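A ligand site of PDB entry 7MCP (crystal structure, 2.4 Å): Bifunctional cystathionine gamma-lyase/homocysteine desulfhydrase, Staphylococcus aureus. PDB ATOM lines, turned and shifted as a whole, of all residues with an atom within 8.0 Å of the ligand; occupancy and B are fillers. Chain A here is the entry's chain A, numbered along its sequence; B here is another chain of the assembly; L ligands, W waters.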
ATOM      1  N   SER A   1      18.094 -20.540   3.707  1.00  0.00           N
ATOM      2  CA  SER A   1      17.101 -21.546   3.994  1.00  0.00           C
ATOM      3  C   SER A   1      16.973 -22.468   2.789  1.00  0.00           C
ATOM      4  O   SER A   1      17.791 -23.361   2.638  1.00  0.00           O
ATOM      5  CB  SER A   1      15.753 -20.910   4.330  1.00  0.00           C
ATOM      6  OG  SER A   1      14.787 -21.929   4.582  1.00  0.00           O
ATOM      7  N   ASN A   2      16.029 -22.215   1.883  1.00  0.00           N
ATOM      8  CA  ASN A   2      15.893 -23.093   0.733  1.00  0.00           C
ATOM      9  C   ASN A   2      16.907 -22.716  -0.352  1.00  0.00           C
ATOM     10  O   ASN A   2      17.483 -21.624  -0.351  1.00  0.00           O
ATOM     11  CB  ASN A   2      14.474 -23.081   0.188  1.00  0.00           C
ATOM     12  CG  ASN A   2      13.475 -23.695   1.172  1.00  0.00           C
ATOM     13  OD1 ASN A   2      13.847 -24.514   2.008  1.00  0.00           O
ATOM     14  ND2 ASN A   2      12.220 -23.293   1.080  1.00  0.00           N
ATOM     15  N   LYS A   3      17.142 -23.664  -1.265  1.00  0.00           N
ATOM     16  CA  LYS A   3      18.271 -23.580  -2.181  1.00  0.00           C
ATOM     17  C   LYS A   3      18.223 -22.305  -3.029  1.00  0.00           C
ATOM     18  O   LYS A   3      19.242 -21.612  -3.172  1.00  0.00           O
ATOM     19  CB  LYS A   3      18.294 -24.818  -3.088  1.00  0.00           C
ATOM     20  CG  LYS A   3      18.364 -26.138  -2.347  1.00  0.00           C
ATOM     21  CD  LYS A   3      18.688 -27.302  -3.284  1.00  0.00           C
ATOM     22  CE  LYS A   3      17.498 -27.686  -4.174  1.00  0.00           C
ATOM     23  NZ  LYS A   3      17.757 -28.903  -5.020  1.00  0.00           N
ATOM     24  N   LYS A   4      17.051 -21.977  -3.575  1.00  0.00           N
ATOM     25  CA  LYS A   4      16.939 -20.783  -4.413  1.00  0.00           C
ATOM     26  C   LYS A   4      17.255 -19.517  -3.643  1.00  0.00           C
ATOM     27  O   LYS A   4      17.779 -18.561  -4.225  1.00  0.00           O
ATOM     28  CB  LYS A   4      15.541 -20.681  -5.019  1.00  0.00           C
ATOM     29  CG  LYS A   4      15.333 -21.596  -6.214  1.00  0.00           C
ATOM     30  CD  LYS A   4      13.877 -21.624  -6.586  1.00  0.00           C
ATOM     31  CE  LYS A   4      13.579 -22.667  -7.604  1.00  0.00           C
ATOM     32  NZ  LYS A   4      12.115 -22.726  -7.917  1.00  0.00           N
ATOM     33  N   THR A   5      16.982 -19.491  -2.347  1.00  0.00           N
ATOM     34  CA  THR A   5      17.346 -18.329  -1.524  1.00  0.00           C
ATOM     35  C   THR A   5      18.848 -18.292  -1.267  1.00  0.00           C
ATOM     36  O   THR A   5      19.497 -17.252  -1.402  1.00  0.00           O
ATOM     37  CB  THR A   5      16.571 -18.398  -0.203  1.00  0.00           C
ATOM     38  OG1 THR A   5      15.165 -18.483  -0.484  1.00  0.00           O
ATOM     39  CG2 THR A   5      16.857 -17.182   0.669  1.00  0.00           C
ATOM     40  N   LYS A   6      19.419 -19.455  -0.903  1.00  0.00           N
ATOM     41  CA  LYS A   6      20.847 -19.577  -0.673  1.00  0.00           C
ATOM     42  C   LYS A   6      21.652 -19.114  -1.885  1.00  0.00           C
ATOM     43  O   LYS A   6      22.694 -18.468  -1.733  1.00  0.00           O
ATOM     44  CB  LYS A   6      21.159 -21.029  -0.323  1.00  0.00           C
ATOM     45  CG  LYS A   6      22.431 -21.279   0.431  1.00  0.00           C
ATOM     46  CD  LYS A   6      22.521 -22.760   0.752  1.00  0.00           C
ATOM     47  CE  LYS A   6      23.888 -23.150   1.287  1.00  0.00           C
ATOM     48  NZ  LYS A   6      23.892 -24.594   1.720  1.00  0.00           N
ATOM     49  N   LEU A   7      21.174 -19.414  -3.096  1.00  0.00           N
ATOM     50  CA  LEU A   7      21.863 -18.974  -4.316  1.00  0.00           C
ATOM     51  C   LEU A   7      21.954 -17.462  -4.400  1.00  0.00           C
ATOM     52  O   LEU A   7      22.913 -16.924  -4.953  1.00  0.00           O
ATOM     53  CB  LEU A   7      21.125 -19.493  -5.558  1.00  0.00           C
ATOM     54  CG  LEU A   7      21.301 -20.983  -5.869  1.00  0.00           C
ATOM     55  CD1 LEU A   7      20.266 -21.451  -6.864  1.00  0.00           C
ATOM     56  CD2 LEU A   7      22.719 -21.232  -6.388  1.00  0.00           C
ATOM     57  N   ILE A   8      20.941 -16.759  -3.888  1.00  0.00           N
ATOM     58  CA  ILE A   8      20.914 -15.311  -3.992  1.00  0.00           C
ATOM     59  C   ILE A   8      21.683 -14.665  -2.844  1.00  0.00           C
ATOM     60  O   ILE A   8      22.436 -13.716  -3.058  1.00  0.00           O
ATOM     61  CB  ILE A   8      19.454 -14.815  -4.059  1.00  0.00           C
ATOM     62  CG1 ILE A   8      18.737 -15.480  -5.228  1.00  0.00           C
ATOM     63  CG2 ILE A   8      19.406 -13.295  -4.158  1.00  0.00           C
ATOM     64  CD1 ILE A   8      19.507 -15.400  -6.538  1.00  0.00           C
ATOM     65  N   HIS A   9      21.536 -15.205  -1.638  1.00  0.00           N
ATOM     66  CA  HIS A   9      22.087 -14.556  -0.447  1.00  0.00           C
ATOM     67  C   HIS A   9      23.273 -15.288   0.149  1.00  0.00           C
ATOM     68  O   HIS A   9      23.878 -14.778   1.094  1.00  0.00           O
ATOM     69  CB  HIS A   9      20.969 -14.371   0.582  1.00  0.00           C
ATOM     70  CG  HIS A   9      19.878 -13.459   0.094  1.00  0.00           C
ATOM     71  ND1 HIS A   9      20.046 -12.100  -0.028  1.00  0.00           N
ATOM     72  CD2 HIS A   9      18.628 -13.730  -0.353  1.00  0.00           C
ATOM     73  CE1 HIS A   9      18.938 -11.563  -0.514  1.00  0.00           C
ATOM     74  NE2 HIS A   9      18.068 -12.536  -0.726  1.00  0.00           N
ATOM     75  N   GLY A  10      23.655 -16.451  -0.382  1.00  0.00           N
ATOM     76  CA  GLY A  10      24.832 -17.132   0.137  1.00  0.00           C
ATOM     77  C   GLY A  10      26.112 -16.517  -0.382  1.00  0.00           C
ATOM     78  O   GLY A  10      26.172 -15.981  -1.487  1.00  0.00           O
ATOM     79  N   GLY A  11      27.158 -16.593   0.429  1.00  0.00           N
ATOM     80  CA  GLY A  11      28.429 -16.015   0.066  1.00  0.00           C
ATOM     81  C   GLY A  11      28.430 -14.503   0.229  1.00  0.00           C
ATOM     82  O   GLY A  11      27.429 -13.867   0.559  1.00  0.00           O
ATOM     83  N   THR A  62      30.096 -21.721   0.167  1.00  0.00           N
ATOM     84  CA  THR A  62      28.759 -21.723   0.760  1.00  0.00           C
ATOM     85  C   THR A  62      27.850 -22.757   0.092  1.00  0.00           C
ATOM     86  O   THR A  62      27.150 -23.521   0.767  1.00  0.00           O
ATOM     87  CB  THR A  62      28.125 -20.324   0.662  1.00  0.00           C
ATOM     88  OG1 THR A  62      28.931 -19.380   1.374  1.00  0.00           O
ATOM     89  CG2 THR A  62      26.748 -20.341   1.261  1.00  0.00           C
ATOM     90  N   LEU A  63      27.849 -22.777  -1.248  1.00  0.00           N
ATOM     91  CA  LEU A  63      26.900 -23.637  -1.958  1.00  0.00           C
ATOM     92  C   LEU A  63      27.209 -25.112  -1.762  1.00  0.00           C
ATOM     93  O   LEU A  63      26.291 -25.939  -1.832  1.00  0.00           O
ATOM     94  CB  LEU A  63      26.895 -23.292  -3.449  1.00  0.00           C
ATOM     95  CG  LEU A  63      26.374 -21.891  -3.803  1.00  0.00           C
ATOM     96  CD1 LEU A  63      26.360 -21.718  -5.308  1.00  0.00           C
ATOM     97  CD2 LEU A  63      24.988 -21.664  -3.207  1.00  0.00           C
ATOM     98  N   GLU A  64      28.472 -25.479  -1.534  1.00  0.00           N
ATOM     99  CA  GLU A  64      28.852 -26.859  -1.315  1.00  0.00           C
ATOM    100  C   GLU A  64      28.973 -27.198   0.167  1.00  0.00           C
ATOM    101  O   GLU A  64      29.416 -28.297   0.501  1.00  0.00           O
ATOM    102  CB  GLU A  64      30.166 -27.165  -2.040  1.00  0.00           C
ATOM    103  CG  GLU A  64      30.050 -27.145  -3.566  1.00  0.00           C
ATOM    104  CD  GLU A  64      29.371 -28.389  -4.115  1.00  0.00           C
ATOM    105  OE1 GLU A  64      28.613 -29.040  -3.362  1.00  0.00           O
ATOM    106  OE2 GLU A  64      29.611 -28.730  -5.307  1.00  0.00           O
ATOM    107  N   ASN A  65      28.550 -26.289   1.058  1.00  0.00           N
ATOM    108  CA  ASN A  65      28.636 -26.485   2.506  1.00  0.00           C
ATOM    109  C   ASN A  65      30.056 -26.792   2.951  1.00  0.00           C
ATOM    110  O   ASN A  65      30.283 -27.652   3.792  1.00  0.00           O
ATOM    111  CB  ASN A  65      27.676 -27.576   2.988  1.00  0.00           C
ATOM    112  CG  ASN A  65      26.227 -27.268   2.647  1.00  0.00           C
ATOM    113  OD1 ASN A  65      25.799 -26.108   2.670  1.00  0.00           O
ATOM    114  ND2 ASN A  65      25.459 -28.305   2.314  1.00  0.00           N
ATOM    115  N   ASN A 181      25.777 -32.576  -3.131  1.00  0.00           N
ATOM    116  CA  ASN A 181      26.766 -31.920  -2.276  1.00  0.00           C
ATOM    117  C   ASN A 181      27.693 -32.966  -1.686  1.00  0.00           C
ATOM    118  O   ASN A 181      27.466 -33.473  -0.586  1.00  0.00           O
ATOM    119  CB  ASN A 181      26.065 -31.095  -1.186  1.00  0.00           C
ATOM    120  CG  ASN A 181      25.168 -29.991  -1.778  1.00  0.00           C
ATOM    121  OD1 ASN A 181      23.963 -29.941  -1.514  1.00  0.00           O
ATOM    122  ND2 ASN A 181      25.746 -29.119  -2.591  1.00  0.00           N
ATOM    123  N   ASP A 184      28.908 -32.961   2.069  1.00  0.00           N
ATOM    124  CA  ASP A 184      27.958 -33.425   3.063  1.00  0.00           C
ATOM    125  C   ASP A 184      28.010 -34.939   3.241  1.00  0.00           C
ATOM    126  O   ASP A 184      27.583 -35.440   4.286  1.00  0.00           O
ATOM    127  CB  ASP A 184      26.530 -33.023   2.675  1.00  0.00           C
ATOM    128  CG  ASP A 184      26.296 -31.532   2.777  1.00  0.00           C
ATOM    129  OD1 ASP A 184      27.133 -30.848   3.393  1.00  0.00           O
ATOM    130  OD2 ASP A 184      25.272 -31.044   2.247  1.00  0.00           O
ATOM    131  N   SER B 316      14.473 -10.787   6.700  1.00  0.00           N
ATOM    132  CA  SER B 316      15.816 -11.288   6.432  1.00  0.00           C
ATOM    133  C   SER B 316      16.165 -11.287   4.948  1.00  0.00           C
ATOM    134  O   SER B 316      17.334 -11.092   4.601  1.00  0.00           O
ATOM    135  CB  SER B 316      15.971 -12.728   6.964  1.00  0.00           C
ATOM    136  OG  SER B 316      15.644 -12.798   8.346  1.00  0.00           O
ATOM    137  N   TYR B 317      15.182 -11.467   4.074  1.00  0.00           N
ATOM    138  CA  TYR B 317      15.422 -11.680   2.659  1.00  0.00           C
ATOM    139  C   TYR B 317      14.948 -10.534   1.768  1.00  0.00           C
ATOM    140  O   TYR B 317      14.916 -10.689   0.545  1.00  0.00           O
ATOM    141  CB  TYR B 317      14.777 -13.000   2.223  1.00  0.00           C
ATOM    142  CG  TYR B 317      15.292 -14.174   3.024  1.00  0.00           C
ATOM    143  CD1 TYR B 317      16.656 -14.400   3.160  1.00  0.00           C
ATOM    144  CD2 TYR B 317      14.415 -15.047   3.665  1.00  0.00           C
ATOM    145  CE1 TYR B 317      17.135 -15.461   3.905  1.00  0.00           C
ATOM    146  CE2 TYR B 317      14.881 -16.120   4.399  1.00  0.00           C
ATOM    147  CZ  TYR B 317      16.244 -16.325   4.515  1.00  0.00           C
ATOM    148  OH  TYR B 317      16.716 -17.392   5.255  1.00  0.00           O
ATOM    149  N   GLU B 364      14.356 -15.443  -5.075  1.00  0.00           N
ATOM    150  CA  GLU B 364      14.548 -16.314  -3.929  1.00  0.00           C
ATOM    151  C   GLU B 364      13.428 -17.331  -3.851  1.00  0.00           C
ATOM    152  O   GLU B 364      12.448 -17.286  -4.614  1.00  0.00           O
ATOM    153  CB  GLU B 364      14.634 -15.515  -2.625  1.00  0.00           C
ATOM    154  CG  GLU B 364      15.773 -14.506  -2.570  1.00  0.00           C
ATOM    155  CD  GLU B 364      15.305 -13.089  -2.910  1.00  0.00           C
ATOM    156  OE1 GLU B 364      14.310 -12.951  -3.659  1.00  0.00           O
ATOM    157  OE2 GLU B 364      15.924 -12.127  -2.425  1.00  0.00           O
ATOM    158  N   ASP B 368      10.347 -19.032   1.359  1.00  0.00           N
ATOM    159  CA  ASP B 368      11.124 -18.110   2.181  1.00  0.00           C
ATOM    160  C   ASP B 368      10.588 -16.692   2.079  1.00  0.00           C
ATOM    161  O   ASP B 368      10.459 -15.995   3.093  1.00  0.00           O
ATOM    162  CB  ASP B 368      12.598 -18.134   1.769  1.00  0.00           C
ATOM    163  CG  ASP B 368      13.274 -19.456   2.086  1.00  0.00           C
ATOM    164  OD1 ASP B 368      12.925 -20.079   3.114  1.00  0.00           O
ATOM    165  OD2 ASP B 368      14.161 -19.857   1.301  1.00  0.00           O
HETATM  166  N1  LIG L   1      23.103 -19.104   3.579  1.00  0.00           N
HETATM  167  C1  LIG L   1      21.971 -18.510   3.153  1.00  0.00           C
HETATM  168  C2  LIG L   1      22.066 -17.141   2.558  1.00  0.00           C
HETATM  169  C3  LIG L   1      20.743 -19.159   3.269  1.00  0.00           C
HETATM  170  O1  LIG L   1      19.621 -18.537   2.820  1.00  0.00           O
HETATM  171  C4  LIG L   1      20.665 -20.434   3.839  1.00  0.00           C
HETATM  172  C5  LIG L   1      19.378 -21.136   3.964  1.00  0.00           C
HETATM  173  C6  LIG L   1      21.860 -21.045   4.265  1.00  0.00           C
HETATM  174  C7  LIG L   1      23.042 -20.321   4.127  1.00  0.00           C
HETATM  175  C8  LIG L   1      21.896 -22.420   4.920  1.00  0.00           C
HETATM  176  O2  LIG L   1      21.612 -23.431   3.945  1.00  0.00           O
HETATM  177  P1  LIG L   1      21.802 -24.975   4.399  1.00  0.00           P
HETATM  178  O3  LIG L   1      23.231 -25.158   4.871  1.00  0.00           O
HETATM  179  O4  LIG L   1      21.537 -25.922   3.246  1.00  0.00           O
HETATM  180  O5  LIG L   1      20.814 -25.265   5.512  1.00  0.00           O
HETATM  181  O   HOH W   1      19.593 -24.943   1.251  1.00  0.00           O
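Water W1 lies within hydrogen-bond range of O of Ser 1 (2.8 Å) and O4 of the ligand (3.0 Å).
Thr 5 touches the ligand. His 9 touches the ligand. Gly 10 touches the ligand. OD1 of Asn 65 touches O3 of the ligand, at 3.5 Å. OH of Tyr 317 of chain B touches O1 of the ligand, at 3.96 Å. Hydrophobic or aromatic side chains within 4 Å of the ligand: His 9. Of the 21 residues printed, 7 come within 4 Å of the ligand. The nearest printed residue that does not touch the ligand is Asn 2 (4.1 Å).
OD1 of Asn 65 sits close to O of Thr 62 (3.5 Å). The side-chain carboxylate (OD2) of Asp 368 of chain B lies within hydrogen-bond range of the side-chain hydroxyl (OG1) of Thr 5 (2.5 Å). OE2 of Glu 364 of chain B sits at hydrogen-bond distance from NE2 of His 9 (2.8 Å). ND2 of Asn 65 is in hydrogen-bond range of OD2 of Asp 184. OG of Ser 1 lies within hydrogen-bond range of OD1 of Asp 368 of chain B, 3.0 Å away. The side-chain amino group (NZ) of Lys 6 is in hydrogen-bond range of the side-chain amide oxygen (OD1) of Asn 65, at 2.6 Å.
The backbone NH (N) of Ser 1 is covalently linked to a carbon (C5) of the ligand, at 1.4 Å. O4 of the ligand is in salt-bridge range of NZ of Lys 6, 3.1 Å away.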
